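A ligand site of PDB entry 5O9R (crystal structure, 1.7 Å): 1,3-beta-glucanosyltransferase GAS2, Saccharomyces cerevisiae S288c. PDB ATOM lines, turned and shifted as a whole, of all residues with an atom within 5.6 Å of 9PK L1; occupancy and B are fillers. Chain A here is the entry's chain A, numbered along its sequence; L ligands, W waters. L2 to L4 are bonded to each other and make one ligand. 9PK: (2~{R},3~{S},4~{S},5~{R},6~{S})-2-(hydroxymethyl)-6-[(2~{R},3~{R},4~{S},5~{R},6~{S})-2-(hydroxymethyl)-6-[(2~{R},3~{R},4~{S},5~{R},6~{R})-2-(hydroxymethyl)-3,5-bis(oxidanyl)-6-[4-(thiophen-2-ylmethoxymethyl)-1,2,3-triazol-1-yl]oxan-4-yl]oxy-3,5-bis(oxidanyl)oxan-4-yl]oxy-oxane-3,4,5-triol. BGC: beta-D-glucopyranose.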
ATOM      1  N   GLN A  60      17.317 -17.584   0.588  1.00  0.00           N
ATOM      2  CA  GLN A  60      18.759 -17.634   0.380  1.00  0.00           C
ATOM      3  C   GLN A  60      19.155 -16.513  -0.570  1.00  0.00           C
ATOM      4  O   GLN A  60      18.660 -16.442  -1.693  1.00  0.00           O
ATOM      5  CB  GLN A  60      19.194 -18.990  -0.202  1.00  0.00           C
ATOM      6  CG  GLN A  60      20.712 -19.184  -0.230  1.00  0.00           C
ATOM      7  CD  GLN A  60      21.298 -19.501   1.131  1.00  0.00           C
ATOM      8  OE1 GLN A  60      20.791 -20.357   1.853  1.00  0.00           O
ATOM      9  NE2 GLN A  60      22.394 -18.840   1.487  1.00  0.00           N
ATOM     10  N   GLN A  62      22.119 -14.370  -2.647  1.00  0.00           N
ATOM     11  CA  GLN A  62      23.412 -14.590  -3.305  1.00  0.00           C
ATOM     12  C   GLN A  62      24.039 -13.244  -3.672  1.00  0.00           C
ATOM     13  O   GLN A  62      23.347 -12.223  -3.739  1.00  0.00           O
ATOM     14  CB  GLN A  62      23.261 -15.514  -4.525  1.00  0.00           C
ATOM     15  CG  GLN A  62      22.789 -14.844  -5.818  1.00  0.00           C
ATOM     16  CD  GLN A  62      22.321 -15.835  -6.879  1.00  0.00           C
ATOM     17  OE1 GLN A  62      21.933 -16.963  -6.578  1.00  0.00           O
ATOM     18  NE2 GLN A  62      22.347 -15.391  -8.131  1.00  0.00           N
ATOM     19  N   TYR A 107      19.902 -22.935   2.045  1.00  0.00           N
ATOM     20  CA  TYR A 107      20.886 -23.767   1.348  1.00  0.00           C
ATOM     21  C   TYR A 107      22.294 -23.654   1.925  1.00  0.00           C
ATOM     22  O   TYR A 107      23.111 -24.553   1.708  1.00  0.00           O
ATOM     23  CB  TYR A 107      20.920 -23.410  -0.141  1.00  0.00           C
ATOM     24  CG  TYR A 107      19.644 -23.722  -0.881  1.00  0.00           C
ATOM     25  CD1 TYR A 107      18.584 -22.819  -0.871  1.00  0.00           C
ATOM     26  CD2 TYR A 107      19.499 -24.900  -1.607  1.00  0.00           C
ATOM     27  CE1 TYR A 107      17.402 -23.091  -1.558  1.00  0.00           C
ATOM     28  CE2 TYR A 107      18.316 -25.180  -2.299  1.00  0.00           C
ATOM     29  CZ  TYR A 107      17.275 -24.268  -2.267  1.00  0.00           C
ATOM     30  OH  TYR A 107      16.104 -24.521  -2.949  1.00  0.00           O
ATOM     31  N   ALA A 108      22.596 -22.563   2.632  1.00  0.00           N
ATOM     32  CA  ALA A 108      23.934 -22.387   3.193  1.00  0.00           C
ATOM     33  C   ALA A 108      23.944 -21.429   4.378  1.00  0.00           C
ATOM     34  O   ALA A 108      23.404 -20.336   4.277  1.00  0.00           O
ATOM     35  CB  ALA A 108      24.900 -21.904   2.122  1.00  0.00           C
ATOM     36  N   ASP A 132      20.368 -27.249   4.280  1.00  0.00           N
ATOM     37  CA  ASP A 132      21.419 -28.053   3.643  1.00  0.00           C
ATOM     38  C   ASP A 132      22.698 -27.965   4.475  1.00  0.00           C
ATOM     39  O   ASP A 132      23.014 -26.916   5.047  1.00  0.00           O
ATOM     40  CB  ASP A 132      21.682 -27.571   2.216  1.00  0.00           C
ATOM     41  CG  ASP A 132      20.485 -27.765   1.289  1.00  0.00           C
ATOM     42  OD1 ASP A 132      19.474 -27.036   1.436  1.00  0.00           O
ATOM     43  OD2 ASP A 132      20.552 -28.636   0.386  1.00  0.00           O
ATOM     44  N   SER A 134      25.737 -28.793   3.148  1.00  0.00           N
ATOM     45  CA  SER A 134      26.797 -28.447   2.201  1.00  0.00           C
ATOM     46  C   SER A 134      26.759 -26.969   1.809  1.00  0.00           C
ATOM     47  O   SER A 134      25.854 -26.227   2.179  1.00  0.00           O
ATOM     48  CB  SER A 134      26.664 -29.327   0.960  1.00  0.00           C
ATOM     49  OG  SER A 134      25.398 -29.115   0.331  1.00  0.00           O
ATOM     50  N   GLU A 135      27.780 -26.562   1.048  1.00  0.00           N
ATOM     51  CA  GLU A 135      27.834 -25.237   0.438  1.00  0.00           C
ATOM     52  C   GLU A 135      28.584 -25.379  -0.893  1.00  0.00           C
ATOM     53  O   GLU A 135      29.255 -26.383  -1.099  1.00  0.00           O
ATOM     54  CB  GLU A 135      28.488 -24.224   1.403  1.00  0.00           C
ATOM     55  CG  GLU A 135      29.938 -24.509   1.777  1.00  0.00           C
ATOM     56  CD  GLU A 135      30.955 -23.598   1.084  1.00  0.00           C
ATOM     57  OE1 GLU A 135      30.700 -23.132  -0.049  1.00  0.00           O
ATOM     58  OE2 GLU A 135      32.029 -23.370   1.684  1.00  0.00           O
ATOM     59  N   PRO A 136      28.452 -24.393  -1.808  1.00  0.00           N
ATOM     60  CA  PRO A 136      29.007 -24.556  -3.167  1.00  0.00           C
ATOM     61  C   PRO A 136      30.468 -25.029  -3.260  1.00  0.00           C
ATOM     62  O   PRO A 136      30.790 -25.829  -4.135  1.00  0.00           O
ATOM     63  CB  PRO A 136      28.841 -23.179  -3.786  1.00  0.00           C
ATOM     64  CG  PRO A 136      27.638 -22.628  -3.099  1.00  0.00           C
ATOM     65  CD  PRO A 136      27.734 -23.111  -1.677  1.00  0.00           C
ATOM     66  N   ASP A 137      31.324 -24.527  -2.367  1.00  0.00           N
ATOM     67  CA  ASP A 137      32.759 -24.905  -2.337  1.00  0.00           C
ATOM     68  C   ASP A 137      33.086 -26.163  -1.510  1.00  0.00           C
ATOM     69  O   ASP A 137      34.186 -26.690  -1.643  1.00  0.00           O
ATOM     70  CB  ASP A 137      33.608 -23.735  -1.837  1.00  0.00           C
ATOM     71  CG  ASP A 137      33.619 -22.547  -2.791  1.00  0.00           C
ATOM     72  OD1 ASP A 137      33.267 -22.703  -3.987  1.00  0.00           O
ATOM     73  OD2 ASP A 137      33.981 -21.440  -2.348  1.00  0.00           O
ATOM     74  N   SER A 139      31.043 -29.500  -1.075  1.00  0.00           N
ATOM     75  CA  SER A 139      29.931 -30.390  -1.410  1.00  0.00           C
ATOM     76  C   SER A 139      30.532 -31.662  -1.988  1.00  0.00           C
ATOM     77  O   SER A 139      31.685 -31.680  -2.424  1.00  0.00           O
ATOM     78  CB  SER A 139      29.054 -29.773  -2.489  1.00  0.00           C
ATOM     79  OG  SER A 139      28.239 -28.731  -1.994  1.00  0.00           O
ATOM     80  N   ILE A 140      29.718 -32.719  -2.040  1.00  0.00           N
ATOM     81  CA  ILE A 140      30.101 -33.927  -2.773  1.00  0.00           C
ATOM     82  C   ILE A 140      30.050 -33.565  -4.254  1.00  0.00           C
ATOM     83  O   ILE A 140      28.994 -33.202  -4.783  1.00  0.00           O
ATOM     84  CB  ILE A 140      29.157 -35.118  -2.457  1.00  0.00           C
ATOM     85  CG1 ILE A 140      29.297 -35.529  -0.987  1.00  0.00           C
ATOM     86  CG2 ILE A 140      29.470 -36.299  -3.369  1.00  0.00           C
ATOM     87  CD1 ILE A 140      28.153 -36.366  -0.465  1.00  0.00           C
ATOM     88  N   ASN A 141      31.210 -33.630  -4.916  1.00  0.00           N
ATOM     89  CA  ASN A 141      31.329 -33.236  -6.324  1.00  0.00           C
ATOM     90  C   ASN A 141      30.805 -34.345  -7.223  1.00  0.00           C
ATOM     91  O   ASN A 141      31.397 -35.414  -7.299  1.00  0.00           O
ATOM     92  CB  ASN A 141      32.805 -32.926  -6.648  1.00  0.00           C
ATOM     93  CG  ASN A 141      32.992 -32.310  -8.032  1.00  0.00           C
ATOM     94  OD1 ASN A 141      32.211 -32.533  -8.945  1.00  0.00           O
ATOM     95  ND2 ASN A 141      34.068 -31.540  -8.175  1.00  0.00           N
ATOM     96  N   ARG A 142      29.698 -34.076  -7.923  1.00  0.00           N
ATOM     97  CA  ARG A 142      29.090 -35.118  -8.764  1.00  0.00           C
ATOM     98  C   ARG A 142      29.995 -35.594  -9.918  1.00  0.00           C
ATOM     99  O   ARG A 142      29.825 -36.720 -10.382  1.00  0.00           O
ATOM    100  CB  ARG A 142      27.724 -34.671  -9.299  1.00  0.00           C
ATOM    101  CG  ARG A 142      27.726 -33.566 -10.351  1.00  0.00           C
ATOM    102  CD  ARG A 142      26.335 -33.314 -10.903  1.00  0.00           C
ATOM    103  NE  ARG A 142      25.436 -32.653  -9.958  1.00  0.00           N
ATOM    104  CZ  ARG A 142      25.338 -31.330  -9.774  1.00  0.00           C
ATOM    105  NH1 ARG A 142      26.112 -30.467 -10.436  1.00  0.00           N
ATOM    106  NH2 ARG A 142      24.460 -30.855  -8.891  1.00  0.00           N
ATOM    107  N   GLU A 143      30.933 -34.748 -10.355  1.00  0.00           N
ATOM    108  CA  GLU A 143      31.902 -35.086 -11.419  1.00  0.00           C
ATOM    109  C   GLU A 143      33.087 -35.922 -10.914  1.00  0.00           C
ATOM    110  O   GLU A 143      33.739 -36.629 -11.709  1.00  0.00           O
ATOM    111  CB  GLU A 143      32.454 -33.810 -12.058  1.00  0.00           C
ATOM    112  CG  GLU A 143      31.408 -32.803 -12.568  1.00  0.00           C
ATOM    113  CD  GLU A 143      30.527 -33.362 -13.663  1.00  0.00           C
ATOM    114  OE1 GLU A 143      30.992 -34.214 -14.451  1.00  0.00           O
ATOM    115  OE2 GLU A 143      29.349 -32.936 -13.744  1.00  0.00           O
ATOM    116  N   ASN A 175      22.130 -32.218  -2.279  1.00  0.00           N
ATOM    117  CA  ASN A 175      21.139 -31.615  -3.167  1.00  0.00           C
ATOM    118  C   ASN A 175      21.504 -31.909  -4.625  1.00  0.00           C
ATOM    119  O   ASN A 175      22.490 -31.379  -5.126  1.00  0.00           O
ATOM    120  CB  ASN A 175      21.044 -30.105  -2.947  1.00  0.00           C
ATOM    121  CG  ASN A 175      19.972 -29.463  -3.808  1.00  0.00           C
ATOM    122  OD1 ASN A 175      18.820 -29.845  -3.746  1.00  0.00           O
ATOM    123  ND2 ASN A 175      20.365 -28.492  -4.630  1.00  0.00           N
ATOM    124  N   GLU A 176      20.727 -32.776  -5.271  1.00  0.00           N
ATOM    125  CA  GLU A 176      20.888 -33.089  -6.698  1.00  0.00           C
ATOM    126  C   GLU A 176      22.327 -33.466  -7.041  1.00  0.00           C
ATOM    127  O   GLU A 176      22.919 -32.901  -7.960  1.00  0.00           O
ATOM    128  CB  GLU A 176      20.477 -31.895  -7.560  1.00  0.00           C
ATOM    129  CG  GLU A 176      19.095 -31.368  -7.269  1.00  0.00           C
ATOM    130  CD  GLU A 176      18.662 -30.293  -8.244  1.00  0.00           C
ATOM    131  OE1 GLU A 176      19.491 -29.751  -9.003  1.00  0.00           O
ATOM    132  OE2 GLU A 176      17.459 -30.012  -8.248  1.00  0.00           O
ATOM    133  N   VAL A 177      22.891 -34.402  -6.279  1.00  0.00           N
ATOM    134  CA  VAL A 177      24.282 -34.804  -6.485  1.00  0.00           C
ATOM    135  C   VAL A 177      24.291 -35.620  -7.785  1.00  0.00           C
ATOM    136  O   VAL A 177      24.707 -35.107  -8.824  1.00  0.00           O
ATOM    137  CB  VAL A 177      24.872 -35.546  -5.271  1.00  0.00           C
ATOM    138  CG1 VAL A 177      26.333 -35.886  -5.500  1.00  0.00           C
ATOM    139  CG2 VAL A 177      24.725 -34.676  -4.021  1.00  0.00           C
ATOM    140  N   TYR A 244       9.123 -29.342 -10.703  1.00  0.00           N
ATOM    141  CA  TYR A 244       8.719 -28.253 -11.607  1.00  0.00           C
ATOM    142  C   TYR A 244       7.782 -28.700 -12.746  1.00  0.00           C
ATOM    143  O   TYR A 244       7.671 -28.028 -13.762  1.00  0.00           O
ATOM    144  CB  TYR A 244       9.968 -27.570 -12.162  1.00  0.00           C
ATOM    145  CG  TYR A 244      10.767 -26.845 -11.102  1.00  0.00           C
ATOM    146  CD1 TYR A 244      10.519 -25.499 -10.827  1.00  0.00           C
ATOM    147  CD2 TYR A 244      11.743 -27.500 -10.366  1.00  0.00           C
ATOM    148  CE1 TYR A 244      11.233 -24.820  -9.854  1.00  0.00           C
ATOM    149  CE2 TYR A 244      12.470 -26.824  -9.389  1.00  0.00           C
ATOM    150  CZ  TYR A 244      12.203 -25.487  -9.135  1.00  0.00           C
ATOM    151  OH  TYR A 244      12.912 -24.803  -8.169  1.00  0.00           O
ATOM    152  N   GLU A 275      11.464 -28.101  -3.597  1.00  0.00           N
ATOM    153  CA  GLU A 275      11.243 -26.895  -4.395  1.00  0.00           C
ATOM    154  C   GLU A 275       9.991 -27.109  -5.254  1.00  0.00           C
ATOM    155  O   GLU A 275       9.708 -28.236  -5.673  1.00  0.00           O
ATOM    156  CB  GLU A 275      12.418 -26.607  -5.321  1.00  0.00           C
ATOM    157  CG  GLU A 275      13.711 -26.185  -4.637  1.00  0.00           C
ATOM    158  CD  GLU A 275      14.911 -26.123  -5.575  1.00  0.00           C
ATOM    159  OE1 GLU A 275      14.729 -26.197  -6.808  1.00  0.00           O
ATOM    160  OE2 GLU A 275      16.041 -25.994  -5.077  1.00  0.00           O
ATOM    161  N   TYR A 307       9.961 -22.017  -4.660  1.00  0.00           N
ATOM    162  CA  TYR A 307      11.257 -21.453  -4.992  1.00  0.00           C
ATOM    163  C   TYR A 307      11.018 -20.159  -5.779  1.00  0.00           C
ATOM    164  O   TYR A 307      10.495 -20.232  -6.886  1.00  0.00           O
ATOM    165  CB  TYR A 307      12.080 -22.442  -5.831  1.00  0.00           C
ATOM    166  CG  TYR A 307      13.478 -21.939  -6.073  1.00  0.00           C
ATOM    167  CD1 TYR A 307      13.763 -21.127  -7.168  1.00  0.00           C
ATOM    168  CD2 TYR A 307      14.515 -22.236  -5.186  1.00  0.00           C
ATOM    169  CE1 TYR A 307      15.051 -20.637  -7.388  1.00  0.00           C
ATOM    170  CE2 TYR A 307      15.798 -21.751  -5.394  1.00  0.00           C
ATOM    171  CZ  TYR A 307      16.060 -20.946  -6.494  1.00  0.00           C
ATOM    172  OH  TYR A 307      17.329 -20.466  -6.711  1.00  0.00           O
ATOM    173  N   MET A 308      11.362 -18.972  -5.251  1.00  0.00           N
ATOM    174  CA  MET A 308      11.887 -18.722  -3.906  1.00  0.00           C
ATOM    175  C   MET A 308      11.490 -17.301  -3.470  1.00  0.00           C
ATOM    176  O   MET A 308      10.783 -16.606  -4.205  1.00  0.00           O
ATOM    177  CB  MET A 308      13.416 -18.884  -3.870  1.00  0.00           C
ATOM    178  CG  MET A 308      14.225 -17.773  -4.551  1.00  0.00           C
ATOM    179  SD  MET A 308      15.826 -17.368  -3.792  1.00  0.00           S
ATOM    180  CE  MET A 308      15.415 -17.213  -2.077  1.00  0.00           C
ATOM    181  N   GLU A 312      16.359 -12.783  -8.205  1.00  0.00           N
ATOM    182  CA  GLU A 312      17.793 -12.655  -8.505  1.00  0.00           C
ATOM    183  C   GLU A 312      18.065 -12.802 -10.003  1.00  0.00           C
ATOM    184  O   GLU A 312      18.841 -13.660 -10.429  1.00  0.00           O
ATOM    185  CB  GLU A 312      18.580 -13.691  -7.688  1.00  0.00           C
ATOM    186  CG  GLU A 312      18.362 -13.539  -6.189  1.00  0.00           C
ATOM    187  CD  GLU A 312      19.193 -14.499  -5.373  1.00  0.00           C
ATOM    188  OE1 GLU A 312      19.728 -14.059  -4.328  1.00  0.00           O
ATOM    189  OE2 GLU A 312      19.311 -15.671  -5.769  1.00  0.00           O
ATOM    190  N   TYR A 316      12.313 -16.018 -10.471  1.00  0.00           N
ATOM    191  CA  TYR A 316      11.818 -16.981  -9.476  1.00  0.00           C
ATOM    192  C   TYR A 316      11.433 -16.356  -8.113  1.00  0.00           C
ATOM    193  O   TYR A 316      10.880 -17.054  -7.272  1.00  0.00           O
ATOM    194  CB  TYR A 316      12.827 -18.117  -9.245  1.00  0.00           C
ATOM    195  CG  TYR A 316      12.826 -19.153 -10.355  1.00  0.00           C
ATOM    196  CD1 TYR A 316      11.760 -20.045 -10.509  1.00  0.00           C
ATOM    197  CD2 TYR A 316      13.885 -19.234 -11.257  1.00  0.00           C
ATOM    198  CE1 TYR A 316      11.752 -20.982 -11.529  1.00  0.00           C
ATOM    199  CE2 TYR A 316      13.891 -20.174 -12.273  1.00  0.00           C
ATOM    200  CZ  TYR A 316      12.831 -21.045 -12.405  1.00  0.00           C
ATOM    201  OH  TYR A 316      12.843 -21.971 -13.427  1.00  0.00           O
HETATM  202  C4  9PK L   1      25.081 -26.807  -2.892  1.00  0.00           C
HETATM  203  C5  9PK L   1      23.600 -26.531  -2.730  1.00  0.00           C
HETATM  204  C6  9PK L   1      23.249 -26.486  -1.241  1.00  0.00           C
HETATM  205  C3  9PK L   1      25.424 -26.845  -4.373  1.00  0.00           C
HETATM  206  CBT 9PK L   1      15.549 -25.237 -13.890  1.00  0.00           C
HETATM  207  CBS 9PK L   1      15.477 -26.319 -14.698  1.00  0.00           C
HETATM  208  CBR 9PK L   1      14.815 -27.361 -14.190  1.00  0.00           C
HETATM  209  SBQ 9PK L   1      14.291 -26.911 -12.671  1.00  0.00           S
HETATM  210  CBP 9PK L   1      14.929 -25.425 -12.714  1.00  0.00           C
HETATM  211  CBN 9PK L   1      14.836 -24.385 -11.592  1.00  0.00           C
HETATM  212  OBO 9PK L   1      15.900 -24.593 -10.664  1.00  0.00           O
HETATM  213  CBM 9PK L   1      15.777 -23.660  -9.592  1.00  0.00           C
HETATM  214  CBL 9PK L   1      17.129 -23.523  -8.883  1.00  0.00           C
HETATM  215  CBH 9PK L   1      17.351 -23.716  -7.591  1.00  0.00           C
HETATM  216  NBK 9PK L   1      18.277 -23.200  -9.454  1.00  0.00           N
HETATM  217  NBJ 9PK L   1      19.136 -23.184  -8.579  1.00  0.00           N
HETATM  218  NBI 9PK L   1      18.649 -23.481  -7.460  1.00  0.00           N
HETATM  219  CAG 9PK L   1      19.408 -23.563  -6.184  1.00  0.00           C
HETATM  220  CAK 9PK L   1      20.874 -23.894  -6.449  1.00  0.00           C
HETATM  221  OBA 9PK L   1      20.965 -25.143  -7.135  1.00  0.00           O
HETATM  222  OAY 9PK L   1      19.318 -22.305  -5.493  1.00  0.00           O
HETATM  223  CAI 9PK L   1      19.906 -22.437  -4.198  1.00  0.00           C
HETATM  224  CAJ 9PK L   1      19.690 -21.141  -3.406  1.00  0.00           C
HETATM  225  OBB 9PK L   1      19.933 -20.017  -4.250  1.00  0.00           O
HETATM  226  CAH 9PK L   1      21.394 -22.691  -4.337  1.00  0.00           C
HETATM  227  OAZ 9PK L   1      21.986 -22.828  -3.034  1.00  0.00           O
HETATM  228  CAL 9PK L   1      21.620 -23.977  -5.128  1.00  0.00           C
HETATM  229  O1  9PK L   1      23.018 -24.150  -5.375  1.00  0.00           O
HETATM  230  C1  9PK L   1      23.471 -25.364  -4.752  1.00  0.00           C
HETATM  231  C2  9PK L   1      24.951 -25.565  -5.047  1.00  0.00           C
HETATM  232  O2  9PK L   1      25.144 -25.659  -6.460  1.00  0.00           O
HETATM  233  O5  9PK L   1      23.269 -25.271  -3.336  1.00  0.00           O
HETATM  234  O6  9PK L   1      24.098 -25.532  -0.579  1.00  0.00           O
HETATM  235  O4  9PK L   1      25.408 -28.063  -2.294  1.00  0.00           O
HETATM  236  O3  9PK L   1      26.850 -26.963  -4.538  1.00  0.00           O
HETATM  237  CAM 9PK L   1      27.130 -27.906  -5.581  1.00  0.00           C
HETATM  238  OBD 9PK L   1      26.678 -29.209  -5.201  1.00  0.00           O
HETATM  239  CAO 9PK L   1      26.852 -30.121  -6.299  1.00  0.00           C
HETATM  240  CAP 9PK L   1      26.250 -31.483  -5.930  1.00  0.00           C
HETATM  241  OBG 9PK L   1      26.690 -31.860  -4.620  1.00  0.00           O
HETATM  242  CAN 9PK L   1      28.331 -30.292  -6.587  1.00  0.00           C
HETATM  243  OBE 9PK L   1      28.502 -31.191  -7.689  1.00  0.00           O
HETATM  244  CAR 9PK L   1      28.937 -28.935  -6.949  1.00  0.00           C
HETATM  245  OBC 9PK L   1      30.353 -29.066  -7.091  1.00  0.00           O
HETATM  246  CAQ 9PK L   1      28.636 -27.946  -5.841  1.00  0.00           C
HETATM  247  OBF 9PK L   1      29.080 -26.633  -6.236  1.00  0.00           O
HETATM  248  C2  BGC L   2       5.817 -31.487 -18.188  1.00  0.00           C
HETATM  249  C3  BGC L   2       6.635 -30.405 -17.483  1.00  0.00           C
HETATM  250  C4  BGC L   2       6.858 -29.294 -18.503  1.00  0.00           C
HETATM  251  C5  BGC L   2       5.486 -28.656 -18.764  1.00  0.00           C
HETATM  252  C6  BGC L   2       5.551 -27.508 -19.758  1.00  0.00           C
HETATM  253  C1  BGC L   2       4.440 -30.855 -18.437  1.00  0.00           C
HETATM  254  O1  BGC L   2       3.570 -31.789 -19.090  1.00  0.00           O
HETATM  255  O2  BGC L   2       5.656 -32.686 -17.433  1.00  0.00           O
HETATM  256  O3  BGC L   2       7.784 -30.786 -16.693  1.00  0.00           O
HETATM  257  O4  BGC L   2       7.804 -28.318 -18.044  1.00  0.00           O
HETATM  258  O5  BGC L   2       4.560 -29.660 -19.239  1.00  0.00           O
HETATM  259  O6  BGC L   2       4.246 -26.954 -19.964  1.00  0.00           O
HETATM  260  C2  BGC L   3       9.890 -31.596 -16.081  1.00  0.00           C
HETATM  261  C3  BGC L   3      10.922 -32.726 -16.050  1.00  0.00           C
HETATM  262  C4  BGC L   3      10.201 -34.049 -15.891  1.00  0.00           C
HETATM  263  C5  BGC L   3       9.170 -34.201 -17.005  1.00  0.00           C
HETATM  264  C6  BGC L   3       8.490 -35.569 -17.022  1.00  0.00           C
HETATM  265  C1  BGC L   3       8.710 -31.844 -17.037  1.00  0.00           C
HETATM  266  O2  BGC L   3      10.558 -30.375 -16.418  1.00  0.00           O
HETATM  267  O3  BGC L   3      11.814 -32.524 -14.937  1.00  0.00           O
HETATM  268  O4  BGC L   3      11.135 -35.129 -15.868  1.00  0.00           O
HETATM  269  O5  BGC L   3       8.193 -33.162 -16.864  1.00  0.00           O
HETATM  270  O6  BGC L   3       7.647 -35.788 -15.890  1.00  0.00           O
HETATM  271  C2  BGC L   4      13.925 -31.808 -14.070  1.00  0.00           C
HETATM  272  C3  BGC L   4      15.388 -31.486 -14.393  1.00  0.00           C
HETATM  273  C4  BGC L   4      15.994 -32.494 -15.362  1.00  0.00           C
HETATM  274  C5  BGC L   4      15.092 -32.697 -16.574  1.00  0.00           C
HETATM  275  C6  BGC L   4      15.637 -33.769 -17.499  1.00  0.00           C
HETATM  276  C1  BGC L   4      13.131 -32.096 -15.338  1.00  0.00           C
HETATM  277  O2  BGC L   4      13.322 -30.731 -13.329  1.00  0.00           O
HETATM  278  O3  BGC L   4      16.128 -31.502 -13.168  1.00  0.00           O
HETATM  279  O4  BGC L   4      17.282 -32.037 -15.769  1.00  0.00           O
HETATM  280  O5  BGC L   4      13.794 -33.079 -16.115  1.00  0.00           O
HETATM  281  O6  BGC L   4      14.718 -33.968 -18.572  1.00  0.00           O
HETATM  282  O   HOH W   1      30.069 -30.390 -10.039  1.00  0.00           O
HETATM  283  O   HOH W   2      20.172 -17.518  -3.888  1.00  0.00           O
HETATM  284  O   HOH W   3      24.312 -22.885  -1.958  1.00  0.00           O
HETATM  285  O   HOH W   4      22.898 -18.776  -4.344  1.00  0.00           O
HETATM  286  O   HOH W   5      16.230 -26.610  -9.075  1.00  0.00           O
HETATM  287  O   HOH W   6      27.258 -24.746  -7.305  1.00  0.00           O
HETATM  288  O   HOH W   7      19.071 -26.880  -9.138  1.00  0.00           O
HETATM  289  O   HOH W   8      23.366 -20.235  -1.804  1.00  0.00           O
HETATM  290  O   HOH W   9      25.018 -31.230  -2.400  1.00  0.00           O
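The backbone carbonyl oxygen of Pro 136 is in hydrogen-bond range of an oxygen (OBF) of 9PK L1, 2.8 Å away.
The backbone carbonyl oxygen of Ser 134 is in hydrogen-bond range of an oxygen (O6) of 9PK L1 (3.3 Å).
The backbone carbonyl oxygen (O) of Ile 140 is in hydrogen-bond range of an oxygen (OBG) of 9PK L1.
The backbone carbonyl oxygen (O) of Tyr 107 lies within hydrogen-bond range of an oxygen (O6) of 9PK L1.
OH of Tyr 307 lies within hydrogen-bond range of OAY of 9PK L1 (3.0 Å).
An oxygen (O4) of 9PK L1 is in hydrogen-bond range of the side-chain hydroxyl of Ser 139, at 2.9 Å.
The side-chain hydroxyl (OG) of Ser 134 is in hydrogen-bond range of an oxygen (O4) of 9PK L1 (2.8 Å).
The backbone NH (N) of Arg 142 sits at hydrogen-bond distance from an oxygen (OBE) of 9PK L1 (3.1 Å).
The guanidinium group (NH2) of Arg 142 is in hydrogen-bond range of the backbone carbonyl oxygen (O) of Glu 176 (2.7 Å).
The backbone carbonyl oxygen (O) of Tyr 316 is in hydrogen-bond range of the backbone NH (N) of Met 308, at 2.8 Å.
OE2 of Glu 275 is in hydrogen-bond range of OH of Tyr 107 (2.6 Å).
The backbone carbonyl oxygen of Val 177 lies within hydrogen-bond range of the guanidinium group of Arg 142, at 2.8 Å.
The backbone NH (N) of Tyr 107 is in hydrogen-bond range of the side-chain amide oxygen (OE1) of Gln 60.
The side-chain amide oxygen of Asn 141 sits at hydrogen-bond distance from the backbone NH of Glu 143 (2.9 Å).
The side-chain carboxylate (OE1) of Glu 135 lies within hydrogen-bond range of the backbone NH (N) of Asp 137 (2.8 Å).
OH of Tyr 244 sits at hydrogen-bond distance from OE1 of Glu 275 (2.7 Å).
CG of Gln 60 touches CAJ of 9PK L1, at 3.9 Å.
Asp 132 touches 9PK L1 (OD2 to C6, 3.8 Å).
CA of Glu 135 touches O6 of 9PK L1 (3.9 Å).
Asn 141 touches 9PK L1.
Asn 175 touches 9PK L1.
Val 177 touches 9PK L1 (CG2 to OBG, 3.5 Å).
Tyr 244 touches 9PK L1 (OH to CBM, 3.4 Å).
Glu 275 touches 9PK L1.
Tyr 316 touches 9PK L1 (OH to CBN, 3.6 Å).
Within 4 Å of 9PK L1: Gln 60, Tyr 107, Asp 132, Ser 134, Glu 135, Pro 136, Ser 139, Ile 140, Asn 141, Arg 142, Asn 175, Val 177, Tyr 244, Glu 275, Tyr 307 and Tyr 316.
Water W5 bridges an oxygen (OBO) of 9PK L1 (2.6 Å) and the side-chain carboxylate of Glu 275 (2.8 Å).
Water W9 lies within hydrogen-bond range of OBG of 9PK L1 (2.8 Å), N of Asn 175 (3.1 Å) and OG of Ser 134 (3.5 Å).
Water W1 bridges OBE of 9PK L1 (2.9 Å) and OD1 of Asn 141 (3.2 Å).
Water W4 lies within hydrogen-bond range of the side-chain amide oxygen (OE1) of Gln 62 and an oxygen (OBB) of 9PK L1.
Water W7 lies within hydrogen-bond range of OE1 of Glu 176 (2.9 Å) and OBA of 9PK L1 (3.3 Å).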
